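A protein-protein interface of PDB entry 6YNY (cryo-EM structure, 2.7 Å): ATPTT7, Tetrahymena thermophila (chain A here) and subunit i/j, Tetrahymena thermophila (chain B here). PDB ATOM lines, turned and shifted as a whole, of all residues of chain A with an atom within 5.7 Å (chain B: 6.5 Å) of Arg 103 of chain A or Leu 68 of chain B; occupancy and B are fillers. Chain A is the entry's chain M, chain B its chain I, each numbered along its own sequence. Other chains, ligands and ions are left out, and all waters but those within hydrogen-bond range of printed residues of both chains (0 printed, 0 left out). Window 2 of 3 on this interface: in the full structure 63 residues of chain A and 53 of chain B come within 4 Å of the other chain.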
ATOM      1  N   ASN A 101      -8.851   9.994 -18.735  1.00  0.00           N
ATOM      2  CA  ASN A 101      -8.715  10.951 -17.645  1.00  0.00           C
ATOM      3  C   ASN A 101      -7.238  11.195 -17.371  1.00  0.00           C
ATOM      4  O   ASN A 101      -6.495  10.261 -17.057  1.00  0.00           O
ATOM      5  CB  ASN A 101      -9.422  10.439 -16.395  1.00  0.00           C
ATOM      6  CG  ASN A 101      -9.584  11.506 -15.343  1.00  0.00           C
ATOM      7  OD1 ASN A 101      -8.696  12.328 -15.130  1.00  0.00           O
ATOM      8  ND2 ASN A 101     -10.728  11.504 -14.681  1.00  0.00           N
ATOM      9  N   ILE A 102      -6.814  12.455 -17.487  1.00  0.00           N
ATOM     10  CA  ILE A 102      -5.406  12.782 -17.321  1.00  0.00           C
ATOM     11  C   ILE A 102      -4.967  12.682 -15.871  1.00  0.00           C
ATOM     12  O   ILE A 102      -3.769  12.560 -15.598  1.00  0.00           O
ATOM     13  CB  ILE A 102      -5.114  14.184 -17.882  1.00  0.00           C
ATOM     14  CG1 ILE A 102      -5.854  15.256 -17.083  1.00  0.00           C
ATOM     15  CG2 ILE A 102      -5.522  14.249 -19.325  1.00  0.00           C
ATOM     16  CD1 ILE A 102      -5.649  16.641 -17.610  1.00  0.00           C
ATOM     17  N   ARG A 103      -5.904  12.727 -14.928  1.00  0.00           N
ATOM     18  CA  ARG A 103      -5.547  12.568 -13.528  1.00  0.00           C
ATOM     19  C   ARG A 103      -5.031  11.173 -13.215  1.00  0.00           C
ATOM     20  O   ARG A 103      -4.471  10.967 -12.134  1.00  0.00           O
ATOM     21  CB  ARG A 103      -6.747  12.879 -12.642  1.00  0.00           C
ATOM     22  CG  ARG A 103      -7.208  14.322 -12.688  1.00  0.00           C
ATOM     23  CD  ARG A 103      -7.879  14.703 -11.394  1.00  0.00           C
ATOM     24  NE  ARG A 103      -9.131  13.991 -11.183  1.00  0.00           N
ATOM     25  CZ  ARG A 103      -9.618  13.665  -9.992  1.00  0.00           C
ATOM     26  NH1 ARG A 103      -8.955  13.969  -8.887  1.00  0.00           N
ATOM     27  NH2 ARG A 103     -10.767  13.020  -9.903  1.00  0.00           N
ATOM     28  N   LEU A 104      -5.207  10.218 -14.127  1.00  0.00           N
ATOM     29  CA  LEU A 104      -4.717   8.858 -13.960  1.00  0.00           C
ATOM     30  C   LEU A 104      -3.609   8.526 -14.951  1.00  0.00           C
ATOM     31  O   LEU A 104      -3.319   7.349 -15.181  1.00  0.00           O
ATOM     32  CB  LEU A 104      -5.873   7.874 -14.107  1.00  0.00           C
ATOM     33  CG  LEU A 104      -6.991   8.038 -13.083  1.00  0.00           C
ATOM     34  CD1 LEU A 104      -8.216   7.279 -13.506  1.00  0.00           C
ATOM     35  CD2 LEU A 104      -6.525   7.572 -11.730  1.00  0.00           C
ATOM     36  N   ARG A 105      -2.980   9.545 -15.536  1.00  0.00           N
ATOM     37  CA  ARG A 105      -1.957   9.312 -16.546  1.00  0.00           C
ATOM     38  C   ARG A 105      -0.786   8.520 -15.982  1.00  0.00           C
ATOM     39  O   ARG A 105      -0.238   7.641 -16.656  1.00  0.00           O
ATOM     40  CB  ARG A 105      -1.478  10.648 -17.108  1.00  0.00           C
ATOM     41  CG  ARG A 105      -0.783  11.517 -16.089  1.00  0.00           C
ATOM     42  CD  ARG A 105      -0.519  12.918 -16.595  1.00  0.00           C
ATOM     43  NE  ARG A 105       0.103  13.740 -15.565  1.00  0.00           N
ATOM     44  CZ  ARG A 105      -0.562  14.310 -14.568  1.00  0.00           C
ATOM     45  NH1 ARG A 105      -1.869  14.149 -14.462  1.00  0.00           N
ATOM     46  NH2 ARG A 105       0.079  15.039 -13.671  1.00  0.00           N
ATOM     47  N   THR A 106      -0.387   8.815 -14.745  1.00  0.00           N
ATOM     48  CA  THR A 106       0.766   8.142 -14.162  1.00  0.00           C
ATOM     49  C   THR A 106       0.536   6.641 -14.071  1.00  0.00           C
ATOM     50  O   THR A 106       1.471   5.850 -14.237  1.00  0.00           O
ATOM     51  CB  THR A 106       1.070   8.729 -12.788  1.00  0.00           C
ATOM     52  OG1 THR A 106       1.398  10.115 -12.922  1.00  0.00           O
ATOM     53  CG2 THR A 106       2.226   8.007 -12.139  1.00  0.00           C
ATOM     54  N   MET A 107      -0.703   6.226 -13.808  1.00  0.00           N
ATOM     55  CA  MET A 107      -1.015   4.804 -13.806  1.00  0.00           C
ATOM     56  C   MET A 107      -0.988   4.243 -15.220  1.00  0.00           C
ATOM     57  O   MET A 107      -0.442   3.161 -15.453  1.00  0.00           O
ATOM     58  CB  MET A 107      -2.376   4.570 -13.156  1.00  0.00           C
ATOM     59  CG  MET A 107      -2.811   3.120 -13.120  1.00  0.00           C
ATOM     60  SD  MET A 107      -1.701   2.062 -12.180  1.00  0.00           S
ATOM     61  CE  MET A 107      -2.196   2.484 -10.518  1.00  0.00           C
ATOM     62  N   MET B  61     -10.592   4.232  -6.763  1.00  0.00           N
ATOM     63  CA  MET B  61     -10.139   4.876  -7.987  1.00  0.00           C
ATOM     64  C   MET B  61     -10.184   6.393  -7.864  1.00  0.00           C
ATOM     65  O   MET B  61      -9.299   7.089  -8.372  1.00  0.00           O
ATOM     66  CB  MET B  61     -10.992   4.412  -9.159  1.00  0.00           C
ATOM     67  CG  MET B  61     -10.426   4.791 -10.483  1.00  0.00           C
ATOM     68  SD  MET B  61     -11.162   3.933 -11.869  1.00  0.00           S
ATOM     69  CE  MET B  61      -9.931   4.362 -13.081  1.00  0.00           C
ATOM     70  N   ALA B  62     -11.212   6.923  -7.202  1.00  0.00           N
ATOM     71  CA  ALA B  62     -11.257   8.355  -6.945  1.00  0.00           C
ATOM     72  C   ALA B  62     -10.071   8.806  -6.107  1.00  0.00           C
ATOM     73  O   ALA B  62      -9.636   9.957  -6.216  1.00  0.00           O
ATOM     74  CB  ALA B  62     -12.567   8.715  -6.252  1.00  0.00           C
ATOM     75  N   PHE B  63      -9.539   7.919  -5.267  1.00  0.00           N
ATOM     76  CA  PHE B  63      -8.341   8.235  -4.501  1.00  0.00           C
ATOM     77  C   PHE B  63      -7.093   8.181  -5.370  1.00  0.00           C
ATOM     78  O   PHE B  63      -6.186   9.002  -5.206  1.00  0.00           O
ATOM     79  CB  PHE B  63      -8.218   7.278  -3.320  1.00  0.00           C
ATOM     80  CG  PHE B  63      -6.837   7.173  -2.768  1.00  0.00           C
ATOM     81  CD1 PHE B  63      -6.256   8.236  -2.115  1.00  0.00           C
ATOM     82  CD2 PHE B  63      -6.122   6.003  -2.891  1.00  0.00           C
ATOM     83  CE1 PHE B  63      -4.990   8.136  -1.609  1.00  0.00           C
ATOM     84  CE2 PHE B  63      -4.855   5.901  -2.383  1.00  0.00           C
ATOM     85  CZ  PHE B  63      -4.290   6.967  -1.741  1.00  0.00           C
ATOM     86  N   GLN B  64      -7.032   7.226  -6.297  1.00  0.00           N
ATOM     87  CA  GLN B  64      -5.900   7.157  -7.214  1.00  0.00           C
ATOM     88  C   GLN B  64      -5.784   8.429  -8.037  1.00  0.00           C
ATOM     89  O   GLN B  64      -4.678   8.919  -8.290  1.00  0.00           O
ATOM     90  CB  GLN B  64      -6.045   5.950  -8.135  1.00  0.00           C
ATOM     91  CG  GLN B  64      -5.973   4.615  -7.447  1.00  0.00           C
ATOM     92  CD  GLN B  64      -6.158   3.469  -8.412  1.00  0.00           C
ATOM     93  OE1 GLN B  64      -7.112   3.440  -9.184  1.00  0.00           O
ATOM     94  NE2 GLN B  64      -5.236   2.522  -8.383  1.00  0.00           N
ATOM     95  N   ALA B  65      -6.918   8.978  -8.466  1.00  0.00           N
ATOM     96  CA  ALA B  65      -6.897  10.178  -9.290  1.00  0.00           C
ATOM     97  C   ALA B  65      -6.327  11.363  -8.524  1.00  0.00           C
ATOM     98  O   ALA B  65      -5.619  12.199  -9.095  1.00  0.00           O
ATOM     99  CB  ALA B  65      -8.305  10.481  -9.788  1.00  0.00           C
ATOM    100  N   VAL B  66      -6.618  11.448  -7.228  1.00  0.00           N
ATOM    101  CA  VAL B  66      -6.087  12.533  -6.413  1.00  0.00           C
ATOM    102  C   VAL B  66      -4.603  12.324  -6.149  1.00  0.00           C
ATOM    103  O   VAL B  66      -3.788  13.239  -6.314  1.00  0.00           O
ATOM    104  CB  VAL B  66      -6.872  12.641  -5.095  1.00  0.00           C
ATOM    105  CG1 VAL B  66      -6.339  13.775  -4.255  1.00  0.00           C
ATOM    106  CG2 VAL B  66      -8.349  12.825  -5.359  1.00  0.00           C
ATOM    107  N   ALA B  67      -4.231  11.114  -5.735  1.00  0.00           N
ATOM    108  CA  ALA B  67      -2.847  10.844  -5.370  1.00  0.00           C
ATOM    109  C   ALA B  67      -1.912  10.918  -6.567  1.00  0.00           C
ATOM    110  O   ALA B  67      -0.749  11.306  -6.416  1.00  0.00           O
ATOM    111  CB  ALA B  67      -2.751   9.473  -4.709  1.00  0.00           C
ATOM    112  N   LEU B  68      -2.389  10.554  -7.751  1.00  0.00           N
ATOM    113  CA  LEU B  68      -1.560  10.558  -8.946  1.00  0.00           C
ATOM    114  C   LEU B  68      -1.529  11.906  -9.647  1.00  0.00           C
ATOM    115  O   LEU B  68      -0.626  12.148 -10.454  1.00  0.00           O
ATOM    116  CB  LEU B  68      -2.054   9.494  -9.926  1.00  0.00           C
ATOM    117  CG  LEU B  68      -2.007   8.052  -9.431  1.00  0.00           C
ATOM    118  CD1 LEU B  68      -2.763   7.146 -10.370  1.00  0.00           C
ATOM    119  CD2 LEU B  68      -0.585   7.592  -9.299  1.00  0.00           C
ATOM    120  N   HIS B  69      -2.487  12.782  -9.356  1.00  0.00           N
ATOM    121  CA  HIS B  69      -2.591  14.082 -10.009  1.00  0.00           C
ATOM    122  C   HIS B  69      -1.913  15.123  -9.124  1.00  0.00           C
ATOM    123  O   HIS B  69      -2.546  15.830  -8.344  1.00  0.00           O
ATOM    124  CB  HIS B  69      -4.052  14.417 -10.269  1.00  0.00           C
ATOM    125  CG  HIS B  69      -4.258  15.584 -11.177  1.00  0.00           C
ATOM    126  ND1 HIS B  69      -3.759  15.625 -12.459  1.00  0.00           N
ATOM    127  CD2 HIS B  69      -4.929  16.744 -10.998  1.00  0.00           C
ATOM    128  CE1 HIS B  69      -4.105  16.764 -13.027  1.00  0.00           C
ATOM    129  NE2 HIS B  69      -4.816  17.461 -12.162  1.00  0.00           N
ATOM    130  N   ARG B  70      -0.593  15.210  -9.255  1.00  0.00           N
ATOM    131  CA  ARG B  70       0.211  16.120  -8.458  1.00  0.00           C
ATOM    132  C   ARG B  70       1.069  16.986  -9.364  1.00  0.00           C
ATOM    133  O   ARG B  70       1.395  16.607 -10.492  1.00  0.00           O
ATOM    134  CB  ARG B  70       1.119  15.361  -7.481  1.00  0.00           C
ATOM    135  CG  ARG B  70       0.397  14.481  -6.486  1.00  0.00           C
ATOM    136  CD  ARG B  70      -0.561  15.272  -5.633  1.00  0.00           C
ATOM    137  NE  ARG B  70      -1.238  14.435  -4.660  1.00  0.00           N
ATOM    138  CZ  ARG B  70      -2.288  14.829  -3.952  1.00  0.00           C
ATOM    139  NH1 ARG B  70      -2.856  14.007  -3.082  1.00  0.00           N
ATOM    140  NH2 ARG B  70      -2.777  16.047  -4.124  1.00  0.00           N
ATOM    141  N   LEU B  95       2.846   9.980  -2.765  1.00  0.00           N
ATOM    142  CA  LEU B  95       1.549   9.348  -2.949  1.00  0.00           C
ATOM    143  C   LEU B  95       1.470   8.605  -4.276  1.00  0.00           C
ATOM    144  O   LEU B  95       0.944   7.487  -4.316  1.00  0.00           O
ATOM    145  CB  LEU B  95       0.435  10.384  -2.847  1.00  0.00           C
ATOM    146  CG  LEU B  95       0.246  10.997  -1.465  1.00  0.00           C
ATOM    147  CD1 LEU B  95      -0.819  12.054  -1.533  1.00  0.00           C
ATOM    148  CD2 LEU B  95      -0.116   9.934  -0.442  1.00  0.00           C
ATOM    149  N   PRO B  96       1.959   9.173  -5.382  1.00  0.00           N
ATOM    150  CA  PRO B  96       1.998   8.380  -6.620  1.00  0.00           C
ATOM    151  C   PRO B  96       2.747   7.071  -6.453  1.00  0.00           C
ATOM    152  O   PRO B  96       2.244   6.014  -6.852  1.00  0.00           O
ATOM    153  CB  PRO B  96       2.686   9.322  -7.615  1.00  0.00           C
ATOM    154  CG  PRO B  96       2.464  10.672  -7.087  1.00  0.00           C
ATOM    155  CD  PRO B  96       2.379  10.564  -5.606  1.00  0.00           C
ATOM    156  N   ALA B  97       3.941   7.114  -5.861  1.00  0.00           N
ATOM    157  CA  ALA B  97       4.694   5.889  -5.621  1.00  0.00           C
ATOM    158  C   ALA B  97       3.953   4.953  -4.681  1.00  0.00           C
ATOM    159  O   ALA B  97       4.093   3.730  -4.784  1.00  0.00           O
ATOM    160  CB  ALA B  97       6.068   6.220  -5.045  1.00  0.00           C
ATOM    161  N   VAL B  99       0.661   4.617  -4.496  1.00  0.00           N
ATOM    162  CA  VAL B  99      -0.453   4.007  -5.210  1.00  0.00           C
ATOM    163  C   VAL B  99       0.049   2.943  -6.172  1.00  0.00           C
ATOM    164  O   VAL B  99      -0.554   1.873  -6.302  1.00  0.00           O
ATOM    165  CB  VAL B  99      -1.266   5.090  -5.936  1.00  0.00           C
ATOM    166  CG1 VAL B  99      -2.326   4.467  -6.810  1.00  0.00           C
ATOM    167  CG2 VAL B  99      -1.890   6.031  -4.940  1.00  0.00           C
ATOM    168  N   LEU B 100       1.152   3.221  -6.867  1.00  0.00           N
ATOM    169  CA  LEU B 100       1.725   2.234  -7.771  1.00  0.00           C
ATOM    170  C   LEU B 100       2.208   1.007  -7.013  1.00  0.00           C
ATOM    171  O   LEU B 100       2.178  -0.106  -7.548  1.00  0.00           O
ATOM    172  CB  LEU B 100       2.865   2.861  -8.566  1.00  0.00           C
ATOM    173  CG  LEU B 100       2.462   4.045  -9.439  1.00  0.00           C
ATOM    174  CD1 LEU B 100       3.680   4.785  -9.935  1.00  0.00           C
ATOM    175  CD2 LEU B 100       1.619   3.577 -10.603  1.00  0.00           C
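OD1 of Asn 101 of chain A is in hydrogen-bond range of N of Arg 103 of chain A. The backbone carbonyl oxygen (O) of Ile 102 of chain A lies within hydrogen-bond range of the guanidinium group (NH1) of Arg 105 of chain A. The guanidinium group (NE) of Arg 70 of chain B sits close to the backbone carbonyl oxygen (O) of Val 66 of chain B (3.3 Å).
Hydrophobic or aromatic side chains of chain A within 4 Å of the printed part of chain B: Leu 104 and Met 107. Of the 15 printed residues of chain B, 8 touch a printed residue of chain A. Hydrophobic or aromatic side chains of chain B that line the printed part of chain A: Met 61, Ala 65, Val 66, Leu 68, His 69 and Leu 100. Along chain B the printed residues that touch a printed residue of chain A span positions 61 to 100. Among the printed residues, 13 pairs touch across the chains. Among the printed residues, no Asp or Glu carboxylate lies within 4 Å of a Lys or Arg side-chain nitrogen of the other chain.
The guanidinium group (NH1) of Arg 105 of chain A lies within hydrogen-bond range of a ring nitrogen (ND1) of His 69 of chain B. O of Ala 65 of chain B lies close to O of Arg 103 of chain A (3.5 Å).
Among the printed residues, merely in contact across the chains: Arg 103 of chain A with Val 66 of chain B (3.8 Å), Arg 103 of chain A with Leu 68 of chain B (3.6 Å), Arg 103 of chain A with His 69 of chain B (3.5 Å), Leu 104 of chain A with Met 61 of chain B (3.4 Å), Leu 104 of chain A with Gln 64 of chain B (3.9 Å), Leu 104 of chain A with Ala 65 of chain B (3.6 Å), Arg 105 of chain A with Arg 70 of chain B (3.8 Å), Thr 106 of chain A with Leu 68 of chain B (3.8 Å), Met 107 of chain A with Gln 64 of chain B (3.7 Å), Met 107 of chain A with Leu 68 of chain B (3.8 Å) and Met 107 of chain A with Leu 100 of chain B (3.97 Å).
Arg 103 of chain A touches just these residues of chain B: Ala 65 (3.5 Å), Val 66 (3.8 Å), Leu 68 (3.6 Å) and His 69 (3.5 Å). Leu 68 of chain B touches three residues of chain A. Of the printed residues of chain B, Met 107 of chain A touches Gln 64 (3.7 Å), Leu 68 (3.8 Å) and Leu 100 (3.97 Å). Printed residues of chain B within 4 Å of Thr 106 of chain A: Leu 68. The nearest residue of chain B that does not touch Arg 103 of chain A is Gln 64 of chain B (4.4 Å).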
